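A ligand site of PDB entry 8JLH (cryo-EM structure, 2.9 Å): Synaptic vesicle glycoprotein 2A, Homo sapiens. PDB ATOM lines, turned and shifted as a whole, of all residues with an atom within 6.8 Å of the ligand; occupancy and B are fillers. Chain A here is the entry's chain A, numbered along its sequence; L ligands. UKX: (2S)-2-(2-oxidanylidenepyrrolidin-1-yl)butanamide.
OH of Tyr 470 lies within hydrogen-bond range of NZ of Lys 702, 2.9 Å away.
OD1 of Asp 678 lies within hydrogen-bond range of N2 of the ligand.
An oxygen (O1) of the ligand lies within hydrogen-bond range of the side-chain hydroxyl (OH) of Tyr 470 (3.0 Å).
Residues that only touch the ligand: Trp 674 (3.1 Å), Trp 308 (3.6 Å), Tyr 469 (3.7 Å), Ile 281 (3.8 Å) and Lys 702 (3.9996 Å).
Hydrophobic or aromatic side chains that line the ligand: Ile 281, Trp 308, Tyr 469 and Trp 674.
Seven residues have an atom within 4 Å of the ligand: Ile 281, Trp 308, Tyr 469, Tyr 470, Trp 674, Asp 678 and Lys 702.
The nearest printed residue that does not touch the ligand is Leu 184 (4.2 Å).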
ATOM      1  N   LEU A 184       3.415  16.034   3.092  1.00  0.00           N
ATOM      2  CA  LEU A 184       3.455  17.047   2.033  1.00  0.00           C
ATOM      3  C   LEU A 184       4.767  17.064   1.267  1.00  0.00           C
ATOM      4  O   LEU A 184       4.780  17.401   0.081  1.00  0.00           O
ATOM      5  CB  LEU A 184       3.205  18.428   2.643  1.00  0.00           C
ATOM      6  CG  LEU A 184       2.204  19.333   1.929  1.00  0.00           C
ATOM      7  CD1 LEU A 184       0.863  18.635   1.838  1.00  0.00           C
ATOM      8  CD2 LEU A 184       2.070  20.634   2.666  1.00  0.00           C
ATOM      9  N   ASP A 187       4.501  14.752  -1.581  1.00  0.00           N
ATOM     10  CA  ASP A 187       3.850  15.391  -2.733  1.00  0.00           C
ATOM     11  C   ASP A 187       4.807  16.322  -3.457  1.00  0.00           C
ATOM     12  O   ASP A 187       4.821  16.373  -4.689  1.00  0.00           O
ATOM     13  CB  ASP A 187       2.614  16.147  -2.270  1.00  0.00           C
ATOM     14  CG  ASP A 187       1.651  16.431  -3.405  1.00  0.00           C
ATOM     15  OD1 ASP A 187       2.087  17.006  -4.427  1.00  0.00           O
ATOM     16  OD2 ASP A 187       0.453  16.103  -3.277  1.00  0.00           O
ATOM     17  N   ILE A 281      -2.398  16.921  -0.114  1.00  0.00           N
ATOM     18  CA  ILE A 281      -2.581  18.325   0.254  1.00  0.00           C
ATOM     19  C   ILE A 281      -3.956  18.580   0.862  1.00  0.00           C
ATOM     20  O   ILE A 281      -4.034  19.175   1.942  1.00  0.00           O
ATOM     21  CB  ILE A 281      -2.319  19.242  -0.947  1.00  0.00           C
ATOM     22  CG1 ILE A 281      -0.849  19.160  -1.368  1.00  0.00           C
ATOM     23  CG2 ILE A 281      -2.670  20.673  -0.601  1.00  0.00           C
ATOM     24  CD1 ILE A 281      -0.531  19.962  -2.602  1.00  0.00           C
ATOM     25  N   PHE A 285      -4.073  19.464   4.895  1.00  0.00           N
ATOM     26  CA  PHE A 285      -4.482  20.784   5.374  1.00  0.00           C
ATOM     27  C   PHE A 285      -5.767  20.700   6.193  1.00  0.00           C
ATOM     28  O   PHE A 285      -5.863  21.297   7.276  1.00  0.00           O
ATOM     29  CB  PHE A 285      -4.639  21.748   4.196  1.00  0.00           C
ATOM     30  CG  PHE A 285      -3.357  22.408   3.797  1.00  0.00           C
ATOM     31  CD1 PHE A 285      -2.827  23.434   4.563  1.00  0.00           C
ATOM     32  CD2 PHE A 285      -2.669  22.013   2.673  1.00  0.00           C
ATOM     33  CE1 PHE A 285      -1.652  24.051   4.204  1.00  0.00           C
ATOM     34  CE2 PHE A 285      -1.497  22.617   2.308  1.00  0.00           C
ATOM     35  CZ  PHE A 285      -0.979  23.640   3.069  1.00  0.00           C
ATOM     36  N   LEU A 304       3.109  25.270   7.073  1.00  0.00           N
ATOM     37  CA  LEU A 304       3.069  23.905   6.573  1.00  0.00           C
ATOM     38  C   LEU A 304       3.454  23.795   5.098  1.00  0.00           C
ATOM     39  O   LEU A 304       3.668  22.681   4.612  1.00  0.00           O
ATOM     40  CB  LEU A 304       1.670  23.314   6.795  1.00  0.00           C
ATOM     41  CG  LEU A 304       1.508  21.798   6.863  1.00  0.00           C
ATOM     42  CD1 LEU A 304       2.404  21.219   7.934  1.00  0.00           C
ATOM     43  CD2 LEU A 304       0.062  21.445   7.155  1.00  0.00           C
ATOM     44  N   CYS A 305       3.564  24.917   4.386  1.00  0.00           N
ATOM     45  CA  CYS A 305       3.936  24.904   2.982  1.00  0.00           C
ATOM     46  C   CYS A 305       5.442  24.943   2.767  1.00  0.00           C
ATOM     47  O   CYS A 305       5.894  24.981   1.621  1.00  0.00           O
ATOM     48  CB  CYS A 305       3.293  26.080   2.245  1.00  0.00           C
ATOM     49  SG  CYS A 305       1.496  26.137   2.368  1.00  0.00           S
ATOM     50  N   TRP A 308       6.738  21.509   1.001  1.00  0.00           N
ATOM     51  CA  TRP A 308       6.666  21.332  -0.442  1.00  0.00           C
ATOM     52  C   TRP A 308       7.977  21.758  -1.103  1.00  0.00           C
ATOM     53  O   TRP A 308       8.549  21.025  -1.930  1.00  0.00           O
ATOM     54  CB  TRP A 308       5.470  22.123  -0.990  1.00  0.00           C
ATOM     55  CG  TRP A 308       5.195  21.937  -2.448  1.00  0.00           C
ATOM     56  CD1 TRP A 308       4.545  20.897  -3.024  1.00  0.00           C
ATOM     57  CD2 TRP A 308       5.532  22.844  -3.501  1.00  0.00           C
ATOM     58  NE1 TRP A 308       4.469  21.085  -4.385  1.00  0.00           N
ATOM     59  CE2 TRP A 308       5.072  22.279  -4.698  1.00  0.00           C
ATOM     60  CE3 TRP A 308       6.197  24.079  -3.546  1.00  0.00           C
ATOM     61  CZ2 TRP A 308       5.241  22.901  -5.939  1.00  0.00           C
ATOM     62  CZ3 TRP A 308       6.368  24.691  -4.765  1.00  0.00           C
ATOM     63  CH2 TRP A 308       5.890  24.106  -5.943  1.00  0.00           C
ATOM     64  N   TRP A 462      -8.710  29.072  -8.097  1.00  0.00           N
ATOM     65  CA  TRP A 462      -7.860  27.894  -8.205  1.00  0.00           C
ATOM     66  C   TRP A 462      -7.468  27.635  -9.646  1.00  0.00           C
ATOM     67  O   TRP A 462      -6.288  27.444  -9.960  1.00  0.00           O
ATOM     68  CB  TRP A 462      -8.578  26.675  -7.609  1.00  0.00           C
ATOM     69  CG  TRP A 462      -8.449  26.559  -6.133  1.00  0.00           C
ATOM     70  CD1 TRP A 462      -9.311  27.047  -5.194  1.00  0.00           C
ATOM     71  CD2 TRP A 462      -7.406  25.895  -5.396  1.00  0.00           C
ATOM     72  NE1 TRP A 462      -8.863  26.743  -3.930  1.00  0.00           N
ATOM     73  CE2 TRP A 462      -7.700  26.035  -4.029  1.00  0.00           C
ATOM     74  CE3 TRP A 462      -6.251  25.204  -5.776  1.00  0.00           C
ATOM     75  CZ2 TRP A 462      -6.877  25.506  -3.039  1.00  0.00           C
ATOM     76  CZ3 TRP A 462      -5.444  24.688  -4.792  1.00  0.00           C
ATOM     77  CH2 TRP A 462      -5.764  24.833  -3.443  1.00  0.00           C
ATOM     78  N   MET A 465      -4.989  30.576 -11.010  1.00  0.00           N
ATOM     79  CA  MET A 465      -3.631  30.542 -10.482  1.00  0.00           C
ATOM     80  C   MET A 465      -2.901  29.271 -10.894  1.00  0.00           C
ATOM     81  O   MET A 465      -1.713  29.318 -11.217  1.00  0.00           O
ATOM     82  CB  MET A 465      -3.635  30.694  -8.969  1.00  0.00           C
ATOM     83  CG  MET A 465      -4.410  31.890  -8.458  1.00  0.00           C
ATOM     84  SD  MET A 465      -3.781  32.502  -6.894  1.00  0.00           S
ATOM     85  CE  MET A 465      -3.145  30.998  -6.176  1.00  0.00           C
ATOM     86  N   TYR A 469       0.529  29.487 -13.048  1.00  0.00           N
ATOM     87  CA  TYR A 469       1.743  29.021 -12.388  1.00  0.00           C
ATOM     88  C   TYR A 469       2.352  27.835 -13.114  1.00  0.00           C
ATOM     89  O   TYR A 469       3.549  27.827 -13.405  1.00  0.00           O
ATOM     90  CB  TYR A 469       1.451  28.671 -10.927  1.00  0.00           C
ATOM     91  CG  TYR A 469       2.624  28.064 -10.199  1.00  0.00           C
ATOM     92  CD1 TYR A 469       3.566  28.875  -9.569  1.00  0.00           C
ATOM     93  CD2 TYR A 469       2.790  26.691 -10.117  1.00  0.00           C
ATOM     94  CE1 TYR A 469       4.629  28.330  -8.897  1.00  0.00           C
ATOM     95  CE2 TYR A 469       3.857  26.140  -9.451  1.00  0.00           C
ATOM     96  CZ  TYR A 469       4.781  26.964  -8.842  1.00  0.00           C
ATOM     97  OH  TYR A 469       5.844  26.419  -8.170  1.00  0.00           O
ATOM     98  N   TYR A 470       1.546  26.820 -13.414  1.00  0.00           N
ATOM     99  CA  TYR A 470       2.101  25.623 -14.038  1.00  0.00           C
ATOM    100  C   TYR A 470       2.534  25.904 -15.477  1.00  0.00           C
ATOM    101  O   TYR A 470       3.576  25.386 -15.915  1.00  0.00           O
ATOM    102  CB  TYR A 470       1.089  24.491 -13.970  1.00  0.00           C
ATOM    103  CG  TYR A 470       1.046  23.833 -12.614  1.00  0.00           C
ATOM    104  CD1 TYR A 470       1.984  22.868 -12.251  1.00  0.00           C
ATOM    105  CD2 TYR A 470       0.083  24.180 -11.670  1.00  0.00           C
ATOM    106  CE1 TYR A 470       1.942  22.268 -11.008  1.00  0.00           C
ATOM    107  CE2 TYR A 470       0.041  23.592 -10.435  1.00  0.00           C
ATOM    108  CZ  TYR A 470       0.976  22.636 -10.109  1.00  0.00           C
ATOM    109  OH  TYR A 470       0.944  22.038  -8.874  1.00  0.00           O
ATOM    110  N   VAL A 616      11.291  30.190  -3.757  1.00  0.00           N
ATOM    111  CA  VAL A 616      10.064  30.098  -2.981  1.00  0.00           C
ATOM    112  C   VAL A 616      10.328  30.459  -1.524  1.00  0.00           C
ATOM    113  O   VAL A 616       9.447  30.992  -0.837  1.00  0.00           O
ATOM    114  CB  VAL A 616       9.460  28.691  -3.143  1.00  0.00           C
ATOM    115  CG1 VAL A 616       8.655  28.280  -1.921  1.00  0.00           C
ATOM    116  CG2 VAL A 616       8.598  28.622  -4.395  1.00  0.00           C
ATOM    117  N   SER A 670       4.815  34.257  -6.542  1.00  0.00           N
ATOM    118  CA  SER A 670       3.500  33.602  -6.512  1.00  0.00           C
ATOM    119  C   SER A 670       3.257  32.765  -5.248  1.00  0.00           C
ATOM    120  O   SER A 670       2.115  32.356  -4.999  1.00  0.00           O
ATOM    121  CB  SER A 670       3.326  32.724  -7.748  1.00  0.00           C
ATOM    122  OG  SER A 670       3.083  33.511  -8.897  1.00  0.00           O
ATOM    123  N   ILE A 671       4.298  32.500  -4.455  1.00  0.00           N
ATOM    124  CA  ILE A 671       4.140  31.565  -3.345  1.00  0.00           C
ATOM    125  C   ILE A 671       3.265  32.155  -2.242  1.00  0.00           C
ATOM    126  O   ILE A 671       2.529  31.423  -1.566  1.00  0.00           O
ATOM    127  CB  ILE A 671       5.517  31.126  -2.818  1.00  0.00           C
ATOM    128  CG1 ILE A 671       5.370  29.863  -1.966  1.00  0.00           C
ATOM    129  CG2 ILE A 671       6.197  32.240  -2.030  1.00  0.00           C
ATOM    130  CD1 ILE A 671       4.845  28.678  -2.746  1.00  0.00           C
ATOM    131  N   SER A 673       0.680  34.121  -2.760  1.00  0.00           N
ATOM    132  CA  SER A 673      -0.673  33.910  -3.252  1.00  0.00           C
ATOM    133  C   SER A 673      -1.123  32.479  -3.003  1.00  0.00           C
ATOM    134  O   SER A 673      -2.262  32.241  -2.590  1.00  0.00           O
ATOM    135  CB  SER A 673      -0.746  34.234  -4.741  1.00  0.00           C
ATOM    136  OG  SER A 673      -2.022  33.919  -5.263  1.00  0.00           O
ATOM    137  N   TRP A 674      -0.238  31.512  -3.263  1.00  0.00           N
ATOM    138  CA  TRP A 674      -0.618  30.117  -3.055  1.00  0.00           C
ATOM    139  C   TRP A 674      -0.879  29.821  -1.589  1.00  0.00           C
ATOM    140  O   TRP A 674      -1.845  29.119  -1.250  1.00  0.00           O
ATOM    141  CB  TRP A 674       0.451  29.189  -3.624  1.00  0.00           C
ATOM    142  CG  TRP A 674       0.316  29.008  -5.101  1.00  0.00           C
ATOM    143  CD1 TRP A 674       1.036  29.636  -6.065  1.00  0.00           C
ATOM    144  CD2 TRP A 674      -0.603  28.152  -5.779  1.00  0.00           C
ATOM    145  NE1 TRP A 674       0.624  29.209  -7.310  1.00  0.00           N
ATOM    146  CE2 TRP A 674      -0.388  28.301  -7.162  1.00  0.00           C
ATOM    147  CE3 TRP A 674      -1.601  27.265  -5.348  1.00  0.00           C
ATOM    148  CZ2 TRP A 674      -1.112  27.606  -8.111  1.00  0.00           C
ATOM    149  CZ3 TRP A 674      -2.325  26.570  -6.296  1.00  0.00           C
ATOM    150  CH2 TRP A 674      -2.075  26.745  -7.665  1.00  0.00           C
ATOM    151  N   ASN A 675      -0.028  30.333  -0.690  1.00  0.00           N
ATOM    152  CA  ASN A 675      -0.254  30.149   0.740  1.00  0.00           C
ATOM    153  C   ASN A 675      -1.587  30.729   1.183  1.00  0.00           C
ATOM    154  O   ASN A 675      -2.363  30.086   1.906  1.00  0.00           O
ATOM    155  CB  ASN A 675       0.890  30.794   1.529  1.00  0.00           C
ATOM    156  CG  ASN A 675       2.159  29.978   1.504  1.00  0.00           C
ATOM    157  OD1 ASN A 675       2.444  29.228   2.430  1.00  0.00           O
ATOM    158  ND2 ASN A 675       2.931  30.138   0.439  1.00  0.00           N
ATOM    159  N   LEU A 677      -4.216  31.296  -0.641  1.00  0.00           N
ATOM    160  CA  LEU A 677      -5.315  30.520  -1.210  1.00  0.00           C
ATOM    161  C   LEU A 677      -5.545  29.234  -0.430  1.00  0.00           C
ATOM    162  O   LEU A 677      -6.690  28.854  -0.190  1.00  0.00           O
ATOM    163  CB  LEU A 677      -5.040  30.209  -2.680  1.00  0.00           C
ATOM    164  CG  LEU A 677      -6.110  29.356  -3.353  1.00  0.00           C
ATOM    165  CD1 LEU A 677      -7.451  30.063  -3.315  1.00  0.00           C
ATOM    166  CD2 LEU A 677      -5.727  29.013  -4.777  1.00  0.00           C
ATOM    167  N   ASP A 678      -4.468  28.552  -0.019  1.00  0.00           N
ATOM    168  CA  ASP A 678      -4.626  27.343   0.787  1.00  0.00           C
ATOM    169  C   ASP A 678      -5.331  27.657   2.100  1.00  0.00           C
ATOM    170  O   ASP A 678      -6.279  26.950   2.494  1.00  0.00           O
ATOM    171  CB  ASP A 678      -3.260  26.708   1.054  1.00  0.00           C
ATOM    172  CG  ASP A 678      -2.687  26.028  -0.158  1.00  0.00           C
ATOM    173  OD1 ASP A 678      -3.456  25.560  -1.014  1.00  0.00           O
ATOM    174  OD2 ASP A 678      -1.441  25.960  -0.263  1.00  0.00           O
ATOM    175  N   PHE A 694     -11.933  20.770  -0.638  1.00  0.00           N
ATOM    176  CA  PHE A 694     -10.514  20.978  -0.892  1.00  0.00           C
ATOM    177  C   PHE A 694      -9.997  20.023  -1.957  1.00  0.00           C
ATOM    178  O   PHE A 694      -9.228  20.418  -2.842  1.00  0.00           O
ATOM    179  CB  PHE A 694      -9.723  20.833   0.411  1.00  0.00           C
ATOM    180  CG  PHE A 694      -8.453  21.655   0.451  1.00  0.00           C
ATOM    181  CD1 PHE A 694      -7.728  21.923  -0.697  1.00  0.00           C
ATOM    182  CD2 PHE A 694      -7.988  22.162   1.652  1.00  0.00           C
ATOM    183  CE1 PHE A 694      -6.568  22.656  -0.642  1.00  0.00           C
ATOM    184  CE2 PHE A 694      -6.828  22.906   1.699  1.00  0.00           C
ATOM    185  CZ  PHE A 694      -6.123  23.153   0.557  1.00  0.00           C
ATOM    186  N   ASN A 698      -8.508  20.953  -5.575  1.00  0.00           N
ATOM    187  CA  ASN A 698      -7.168  20.503  -5.959  1.00  0.00           C
ATOM    188  C   ASN A 698      -7.189  19.730  -7.268  1.00  0.00           C
ATOM    189  O   ASN A 698      -6.264  19.832  -8.076  1.00  0.00           O
ATOM    190  CB  ASN A 698      -6.566  19.656  -4.831  1.00  0.00           C
ATOM    191  CG  ASN A 698      -5.101  19.920  -4.630  1.00  0.00           C
ATOM    192  OD1 ASN A 698      -4.678  21.062  -4.484  1.00  0.00           O
ATOM    193  ND2 ASN A 698      -4.300  18.869  -4.614  1.00  0.00           N
ATOM    194  N   CYS A 701      -7.303  22.256  -9.820  1.00  0.00           N
ATOM    195  CA  CYS A 701      -5.969  22.814  -9.959  1.00  0.00           C
ATOM    196  C   CYS A 701      -5.098  21.928 -10.855  1.00  0.00           C
ATOM    197  O   CYS A 701      -4.344  22.430 -11.691  1.00  0.00           O
ATOM    198  CB  CYS A 701      -5.336  22.983  -8.584  1.00  0.00           C
ATOM    199  SG  CYS A 701      -3.536  23.141  -8.591  1.00  0.00           S
ATOM    200  N   LYS A 702      -5.188  20.618 -10.680  1.00  0.00           N
ATOM    201  CA  LYS A 702      -4.386  19.705 -11.486  1.00  0.00           C
ATOM    202  C   LYS A 702      -4.836  19.706 -12.951  1.00  0.00           C
ATOM    203  O   LYS A 702      -4.007  19.627 -13.858  1.00  0.00           O
ATOM    204  CB  LYS A 702      -4.435  18.293 -10.905  1.00  0.00           C
ATOM    205  CG  LYS A 702      -3.788  18.198  -9.544  1.00  0.00           C
ATOM    206  CD  LYS A 702      -2.468  18.929  -9.518  1.00  0.00           C
ATOM    207  CE  LYS A 702      -1.830  18.886  -8.145  1.00  0.00           C
ATOM    208  NZ  LYS A 702      -0.631  19.765  -8.080  1.00  0.00           N
HETATM  209  O1  UKX L   1       0.624  22.941  -5.998  1.00  0.00           O
HETATM  210  O2  UKX L   1      -0.722  25.646  -2.853  1.00  0.00           O
HETATM  211  N1  UKX L   1       1.343  24.349  -4.318  1.00  0.00           N
HETATM  212  C1  UKX L   1       1.250  23.916  -5.635  1.00  0.00           C
HETATM  213  C2  UKX L   1       2.031  24.833  -6.534  1.00  0.00           C
HETATM  214  C3  UKX L   1       2.716  25.842  -5.637  1.00  0.00           C
HETATM  215  C4  UKX L   1       2.182  25.566  -4.221  1.00  0.00           C
HETATM  216  C5  UKX L   1      -0.606  24.444  -2.888  1.00  0.00           C
HETATM  217  C6  UKX L   1       0.732  23.734  -3.147  1.00  0.00           C
HETATM  218  C7  UKX L   1       1.586  23.897  -1.874  1.00  0.00           C
HETATM  219  C8  UKX L   1       1.543  22.672  -0.975  1.00  0.00           C
HETATM  220  N2  UKX L   1      -1.730  23.651  -2.685  1.00  0.00           N
